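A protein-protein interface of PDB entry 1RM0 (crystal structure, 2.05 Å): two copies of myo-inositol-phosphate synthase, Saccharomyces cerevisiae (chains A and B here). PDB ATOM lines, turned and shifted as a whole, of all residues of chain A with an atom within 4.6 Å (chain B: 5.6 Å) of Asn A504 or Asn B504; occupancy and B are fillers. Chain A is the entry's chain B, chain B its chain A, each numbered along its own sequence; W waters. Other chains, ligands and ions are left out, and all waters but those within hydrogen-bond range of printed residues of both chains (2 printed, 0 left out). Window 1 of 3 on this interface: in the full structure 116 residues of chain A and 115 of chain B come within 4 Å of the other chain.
CG1 of Val A331 touches CG1 of Val B331, at 3.6 Å.
CD1 of Phe B335 touches CG2 of Val A331, 3.8 Å away.
Phe B335 touches Leu A503 (CE1 to CD2, 3.1 Å).
Asn B504 touches one residue of chain A.
Of the printed residues of chain A, Phe B335 touches Val A331 (3.8 Å) and Leu A503 (3.1 Å).
Printed residues of chain B within 4 Å of Arg A507: Asp B338 (3.2 Å).
Printed residues of chain A within 4 Å of Val B331: Val A331.
Printed residues of chain B within 4 Å of Val A331: Val B331 (3.6 Å) and Phe B335 (3.8 Å).
The nearest printed residue of chain B that does not touch Arg A507 is Phe B335 (6.7 Å).
Val A331 touches its own counterpart, Val B331.
Asn B504 touches its own counterpart, Asn A504.
Of the 5 pairs that touch across the chains among the printed residues, 2 have their exchanged pair printed and touching as well.
Printed residues of chain B that touch a printed residue of chain A: Val B331, Phe B335, Asp B338 and Asn B504.
Hydrophobic or aromatic side chains of chain B that line the printed part of chain A: Val B331 and Phe B335.
Among the printed residues, 5 pairs touch across the chains.
The side-chain hydroxyl (OG1) of Thr B508 sits at hydrogen-bond distance from the backbone carbonyl oxygen (O) of Asn B504.
The backbone carbonyl oxygen (O) of Asn A504 sits at hydrogen-bond distance from the side-chain hydroxyl (OG1) of Thr A508 (2.8 Å).
Water W2 bridges the backbone carbonyl oxygen (O) of Val A331 (2.9 Å) and the side-chain amide oxygen (OD1) of Asn B504 (3.3 Å).
Water W1 lies within hydrogen-bond range of ND2 of Asn B504 (2.9 Å), O of Val B331 (3.0 Å) and ND2 of Asn A504 (3.2 Å).
The guanidinium group of Arg A507 lies within hydrogen-bond range of the backbone carbonyl oxygen of Asp B338, at 3.2 Å.
ND2 of Asn B504 sits close to ND2 of Asn A504 (3.1 Å).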
ATOM      1  N   VAL A 331     -24.045  10.062   4.037  1.00  0.00           N
ATOM      2  CA  VAL A 331     -23.365   9.382   5.134  1.00  0.00           C
ATOM      3  C   VAL A 331     -23.524  10.174   6.438  1.00  0.00           C
ATOM      4  O   VAL A 331     -24.001   9.634   7.435  1.00  0.00           O
ATOM      5  CB  VAL A 331     -21.863   9.207   4.815  1.00  0.00           C
ATOM      6  CG1 VAL A 331     -21.159   8.468   5.939  1.00  0.00           C
ATOM      7  CG2 VAL A 331     -21.708   8.448   3.519  1.00  0.00           C
ATOM      8  N   GLY A 502     -28.922   5.349   1.346  1.00  0.00           N
ATOM      9  CA  GLY A 502     -27.951   5.181   2.414  1.00  0.00           C
ATOM     10  C   GLY A 502     -26.723   4.509   1.839  1.00  0.00           C
ATOM     11  O   GLY A 502     -26.681   3.289   1.703  1.00  0.00           O
ATOM     12  N   LEU A 503     -25.726   5.313   1.487  1.00  0.00           N
ATOM     13  CA  LEU A 503     -24.496   4.808   0.893  1.00  0.00           C
ATOM     14  C   LEU A 503     -23.979   3.534   1.554  1.00  0.00           C
ATOM     15  O   LEU A 503     -23.685   2.552   0.869  1.00  0.00           O
ATOM     16  CB  LEU A 503     -23.403   5.873   0.951  1.00  0.00           C
ATOM     17  CG  LEU A 503     -22.178   5.584   0.085  1.00  0.00           C
ATOM     18  CD1 LEU A 503     -22.461   5.984  -1.367  1.00  0.00           C
ATOM     19  CD2 LEU A 503     -20.995   6.353   0.621  1.00  0.00           C
ATOM     20  N   ASN A 504     -23.859   3.553   2.881  1.00  0.00           N
ATOM     21  CA  ASN A 504     -23.366   2.386   3.611  1.00  0.00           C
ATOM     22  C   ASN A 504     -24.267   1.178   3.368  1.00  0.00           C
ATOM     23  O   ASN A 504     -23.788   0.053   3.238  1.00  0.00           O
ATOM     24  CB  ASN A 504     -23.256   2.690   5.115  1.00  0.00           C
ATOM     25  CG  ASN A 504     -21.983   3.469   5.466  1.00  0.00           C
ATOM     26  OD1 ASN A 504     -21.777   4.588   5.000  1.00  0.00           O
ATOM     27  ND2 ASN A 504     -21.128   2.870   6.290  1.00  0.00           N
ATOM     28  N   LYS A 505     -25.571   1.418   3.299  1.00  0.00           N
ATOM     29  CA  LYS A 505     -26.517   0.347   3.035  1.00  0.00           C
ATOM     30  C   LYS A 505     -26.281  -0.134   1.601  1.00  0.00           C
ATOM     31  O   LYS A 505     -26.224  -1.335   1.337  1.00  0.00           O
ATOM     32  CB  LYS A 505     -27.950   0.858   3.204  1.00  0.00           C
ATOM     33  CG  LYS A 505     -28.332   1.122   4.654  1.00  0.00           C
ATOM     34  CD  LYS A 505     -29.741   1.686   4.792  1.00  0.00           C
ATOM     35  CE  LYS A 505     -29.824   3.106   4.254  1.00  0.00           C
ATOM     36  NZ  LYS A 505     -31.151   3.744   4.505  1.00  0.00           N
ATOM     37  N   GLN A 506     -26.124   0.814   0.683  1.00  0.00           N
ATOM     38  CA  GLN A 506     -25.887   0.495  -0.717  1.00  0.00           C
ATOM     39  C   GLN A 506     -24.618  -0.333  -0.904  1.00  0.00           C
ATOM     40  O   GLN A 506     -24.566  -1.196  -1.777  1.00  0.00           O
ATOM     41  CB  GLN A 506     -25.820   1.783  -1.545  1.00  0.00           C
ATOM     42  CG  GLN A 506     -27.180   2.489  -1.685  1.00  0.00           C
ATOM     43  CD  GLN A 506     -27.106   3.825  -2.424  1.00  0.00           C
ATOM     44  OE1 GLN A 506     -28.132   4.400  -2.795  1.00  0.00           O
ATOM     45  NE2 GLN A 506     -25.892   4.327  -2.624  1.00  0.00           N
ATOM     46  N   ARG A 507     -23.592  -0.086  -0.094  1.00  0.00           N
ATOM     47  CA  ARG A 507     -22.369  -0.873  -0.222  1.00  0.00           C
ATOM     48  C   ARG A 507     -22.590  -2.213   0.471  1.00  0.00           C
ATOM     49  O   ARG A 507     -21.975  -3.213   0.115  1.00  0.00           O
ATOM     50  CB  ARG A 507     -21.159  -0.155   0.398  1.00  0.00           C
ATOM     51  CG  ARG A 507     -19.834  -0.896   0.175  1.00  0.00           C
ATOM     52  CD  ARG A 507     -18.640  -0.091   0.672  1.00  0.00           C
ATOM     53  NE  ARG A 507     -17.343  -0.663   0.289  1.00  0.00           N
ATOM     54  CZ  ARG A 507     -16.710  -1.636   0.947  1.00  0.00           C
ATOM     55  NH1 ARG A 507     -15.536  -2.086   0.516  1.00  0.00           N
ATOM     56  NH2 ARG A 507     -17.243  -2.158   2.045  1.00  0.00           N
ATOM     57  N   THR A 508     -23.475  -2.226   1.462  1.00  0.00           N
ATOM     58  CA  THR A 508     -23.785  -3.449   2.188  1.00  0.00           C
ATOM     59  C   THR A 508     -24.413  -4.450   1.224  1.00  0.00           C
ATOM     60  O   THR A 508     -24.022  -5.616   1.190  1.00  0.00           O
ATOM     61  CB  THR A 508     -24.757  -3.172   3.361  1.00  0.00           C
ATOM     62  OG1 THR A 508     -24.052  -2.503   4.412  1.00  0.00           O
ATOM     63  CG2 THR A 508     -25.343  -4.467   3.903  1.00  0.00           C
ATOM     64  N   SER B 330     -14.964   8.389  13.135  1.00  0.00           N
ATOM     65  CA  SER B 330     -15.129   6.944  12.986  1.00  0.00           C
ATOM     66  C   SER B 330     -16.156   6.623  11.902  1.00  0.00           C
ATOM     67  O   SER B 330     -16.447   5.458  11.629  1.00  0.00           O
ATOM     68  CB  SER B 330     -15.550   6.306  14.322  1.00  0.00           C
ATOM     69  OG  SER B 330     -16.799   6.794  14.786  1.00  0.00           O
ATOM     70  N   VAL B 331     -16.704   7.671  11.298  1.00  0.00           N
ATOM     71  CA  VAL B 331     -17.687   7.533  10.233  1.00  0.00           C
ATOM     72  C   VAL B 331     -17.033   7.977   8.934  1.00  0.00           C
ATOM     73  O   VAL B 331     -17.114   7.298   7.912  1.00  0.00           O
ATOM     74  CB  VAL B 331     -18.938   8.432  10.475  1.00  0.00           C
ATOM     75  CG1 VAL B 331     -19.830   8.442   9.237  1.00  0.00           C
ATOM     76  CG2 VAL B 331     -19.724   7.933  11.669  1.00  0.00           C
ATOM     77  N   GLN B 334     -13.779   5.812   7.893  1.00  0.00           N
ATOM     78  CA  GLN B 334     -14.260   4.511   7.461  1.00  0.00           C
ATOM     79  C   GLN B 334     -14.768   4.679   6.028  1.00  0.00           C
ATOM     80  O   GLN B 334     -14.377   3.950   5.119  1.00  0.00           O
ATOM     81  CB  GLN B 334     -15.418   4.068   8.360  1.00  0.00           C
ATOM     82  CG  GLN B 334     -15.897   2.650   8.140  1.00  0.00           C
ATOM     83  CD  GLN B 334     -14.884   1.626   8.596  1.00  0.00           C
ATOM     84  OE1 GLN B 334     -14.002   1.219   7.835  1.00  0.00           O
ATOM     85  NE2 GLN B 334     -14.991   1.214   9.854  1.00  0.00           N
ATOM     86  N   PHE B 335     -15.650   5.654   5.850  1.00  0.00           N
ATOM     87  CA  PHE B 335     -16.223   5.964   4.555  1.00  0.00           C
ATOM     88  C   PHE B 335     -15.138   6.085   3.470  1.00  0.00           C
ATOM     89  O   PHE B 335     -15.214   5.432   2.424  1.00  0.00           O
ATOM     90  CB  PHE B 335     -17.024   7.265   4.683  1.00  0.00           C
ATOM     91  CG  PHE B 335     -17.300   7.951   3.378  1.00  0.00           C
ATOM     92  CD1 PHE B 335     -18.239   7.443   2.491  1.00  0.00           C
ATOM     93  CD2 PHE B 335     -16.602   9.102   3.030  1.00  0.00           C
ATOM     94  CE1 PHE B 335     -18.477   8.073   1.272  1.00  0.00           C
ATOM     95  CE2 PHE B 335     -16.829   9.739   1.819  1.00  0.00           C
ATOM     96  CZ  PHE B 335     -17.769   9.223   0.936  1.00  0.00           C
ATOM     97  N   ASP B 338     -13.442   2.734   2.723  1.00  0.00           N
ATOM     98  CA  ASP B 338     -14.391   1.809   2.114  1.00  0.00           C
ATOM     99  C   ASP B 338     -14.556   2.149   0.634  1.00  0.00           C
ATOM    100  O   ASP B 338     -14.913   1.290  -0.177  1.00  0.00           O
ATOM    101  CB  ASP B 338     -15.759   1.919   2.784  1.00  0.00           C
ATOM    102  CG  ASP B 338     -15.804   1.260   4.141  1.00  0.00           C
ATOM    103  OD1 ASP B 338     -16.820   1.458   4.850  1.00  0.00           O
ATOM    104  OD2 ASP B 338     -14.839   0.540   4.494  1.00  0.00           O
ATOM    105  N   GLY B 502     -15.468   1.125  13.840  1.00  0.00           N
ATOM    106  CA  GLY B 502     -16.418   1.586  12.845  1.00  0.00           C
ATOM    107  C   GLY B 502     -17.759   1.815  13.504  1.00  0.00           C
ATOM    108  O   GLY B 502     -18.416   0.858  13.919  1.00  0.00           O
ATOM    109  N   LEU B 503     -18.159   3.080  13.607  1.00  0.00           N
ATOM    110  CA  LEU B 503     -19.423   3.440  14.242  1.00  0.00           C
ATOM    111  C   LEU B 503     -20.621   2.678  13.673  1.00  0.00           C
ATOM    112  O   LEU B 503     -21.364   2.030  14.412  1.00  0.00           O
ATOM    113  CB  LEU B 503     -19.689   4.944  14.111  1.00  0.00           C
ATOM    114  CG  LEU B 503     -20.833   5.418  15.017  1.00  0.00           C
ATOM    115  CD1 LEU B 503     -20.290   5.637  16.434  1.00  0.00           C
ATOM    116  CD2 LEU B 503     -21.452   6.700  14.479  1.00  0.00           C
ATOM    117  N   ASN B 504     -20.814   2.769  12.359  1.00  0.00           N
ATOM    118  CA  ASN B 504     -21.935   2.094  11.715  1.00  0.00           C
ATOM    119  C   ASN B 504     -21.942   0.592  11.976  1.00  0.00           C
ATOM    120  O   ASN B 504     -23.009  -0.005  12.112  1.00  0.00           O
ATOM    121  CB  ASN B 504     -21.931   2.374  10.211  1.00  0.00           C
ATOM    122  CG  ASN B 504     -22.153   3.845   9.895  1.00  0.00           C
ATOM    123  OD1 ASN B 504     -23.006   4.502  10.502  1.00  0.00           O
ATOM    124  ND2 ASN B 504     -21.390   4.369   8.935  1.00  0.00           N
ATOM    125  N   LYS B 505     -20.756  -0.014  12.048  1.00  0.00           N
ATOM    126  CA  LYS B 505     -20.647  -1.450  12.322  1.00  0.00           C
ATOM    127  C   LYS B 505     -20.991  -1.748  13.773  1.00  0.00           C
ATOM    128  O   LYS B 505     -21.546  -2.803  14.074  1.00  0.00           O
ATOM    129  CB  LYS B 505     -19.235  -1.963  12.027  1.00  0.00           C
ATOM    130  CG  LYS B 505     -18.965  -2.185  10.548  1.00  0.00           C
ATOM    131  CD  LYS B 505     -17.588  -2.776  10.308  1.00  0.00           C
ATOM    132  CE  LYS B 505     -16.477  -1.797  10.643  1.00  0.00           C
ATOM    133  NZ  LYS B 505     -15.136  -2.376  10.321  1.00  0.00           N
ATOM    134  N   GLN B 506     -20.656  -0.814  14.664  1.00  0.00           N
ATOM    135  CA  GLN B 506     -20.940  -0.973  16.087  1.00  0.00           C
ATOM    136  C   GLN B 506     -22.438  -0.897  16.315  1.00  0.00           C
ATOM    137  O   GLN B 506     -22.985  -1.634  17.141  1.00  0.00           O
ATOM    138  CB  GLN B 506     -20.238   0.116  16.908  1.00  0.00           C
ATOM    139  CG  GLN B 506     -18.719   0.138  16.735  1.00  0.00           C
ATOM    140  CD  GLN B 506     -18.063   1.307  17.445  1.00  0.00           C
ATOM    141  OE1 GLN B 506     -18.574   2.429  17.421  1.00  0.00           O
ATOM    142  NE2 GLN B 506     -16.917   1.055  18.067  1.00  0.00           N
ATOM    143  N   ARG B 507     -23.112  -0.015  15.580  1.00  0.00           N
ATOM    144  CA  ARG B 507     -24.554   0.111  15.748  1.00  0.00           C
ATOM    145  C   ARG B 507     -25.254  -1.113  15.162  1.00  0.00           C
ATOM    146  O   ARG B 507     -26.238  -1.606  15.722  1.00  0.00           O
ATOM    147  CB  ARG B 507     -25.084   1.393  15.081  1.00  0.00           C
ATOM    148  CG  ARG B 507     -26.598   1.583  15.256  1.00  0.00           C
ATOM    149  CD  ARG B 507     -27.046   2.986  14.906  1.00  0.00           C
ATOM    150  NE  ARG B 507     -28.418   3.245  15.341  1.00  0.00           N
ATOM    151  CZ  ARG B 507     -29.506   3.045  14.597  1.00  0.00           C
ATOM    152  NH1 ARG B 507     -29.399   2.575  13.363  1.00  0.00           N
ATOM    153  NH2 ARG B 507     -30.708   3.338  15.080  1.00  0.00           N
ATOM    154  N   THR B 508     -24.739  -1.600  14.035  1.00  0.00           N
ATOM    155  CA  THR B 508     -25.312  -2.767  13.377  1.00  0.00           C
ATOM    156  C   THR B 508     -25.328  -3.969  14.328  1.00  0.00           C
ATOM    157  O   THR B 508     -26.303  -4.722  14.360  1.00  0.00           O
ATOM    158  CB  THR B 508     -24.521  -3.125  12.099  1.00  0.00           C
ATOM    159  OG1 THR B 508     -24.716  -2.101  11.114  1.00  0.00           O
ATOM    160  CG2 THR B 508     -24.990  -4.458  11.537  1.00  0.00           C
ATOM    161  N   ALA B 509     -24.255  -4.136  15.105  1.00  0.00           N
ATOM    162  CA  ALA B 509     -24.154  -5.234  16.066  1.00  0.00           C
ATOM    163  C   ALA B 509     -25.310  -5.143  17.051  1.00  0.00           C
ATOM    164  O   ALA B 509     -25.965  -6.140  17.349  1.00  0.00           O
ATOM    165  CB  ALA B 509     -22.829  -5.169  16.813  1.00  0.00           C
HETATM  166  O   HOH W   1     -18.912   4.938   7.443  1.00  0.00           O
HETATM  167  O   HOH W   2     -23.633   6.903   8.340  1.00  0.00           O
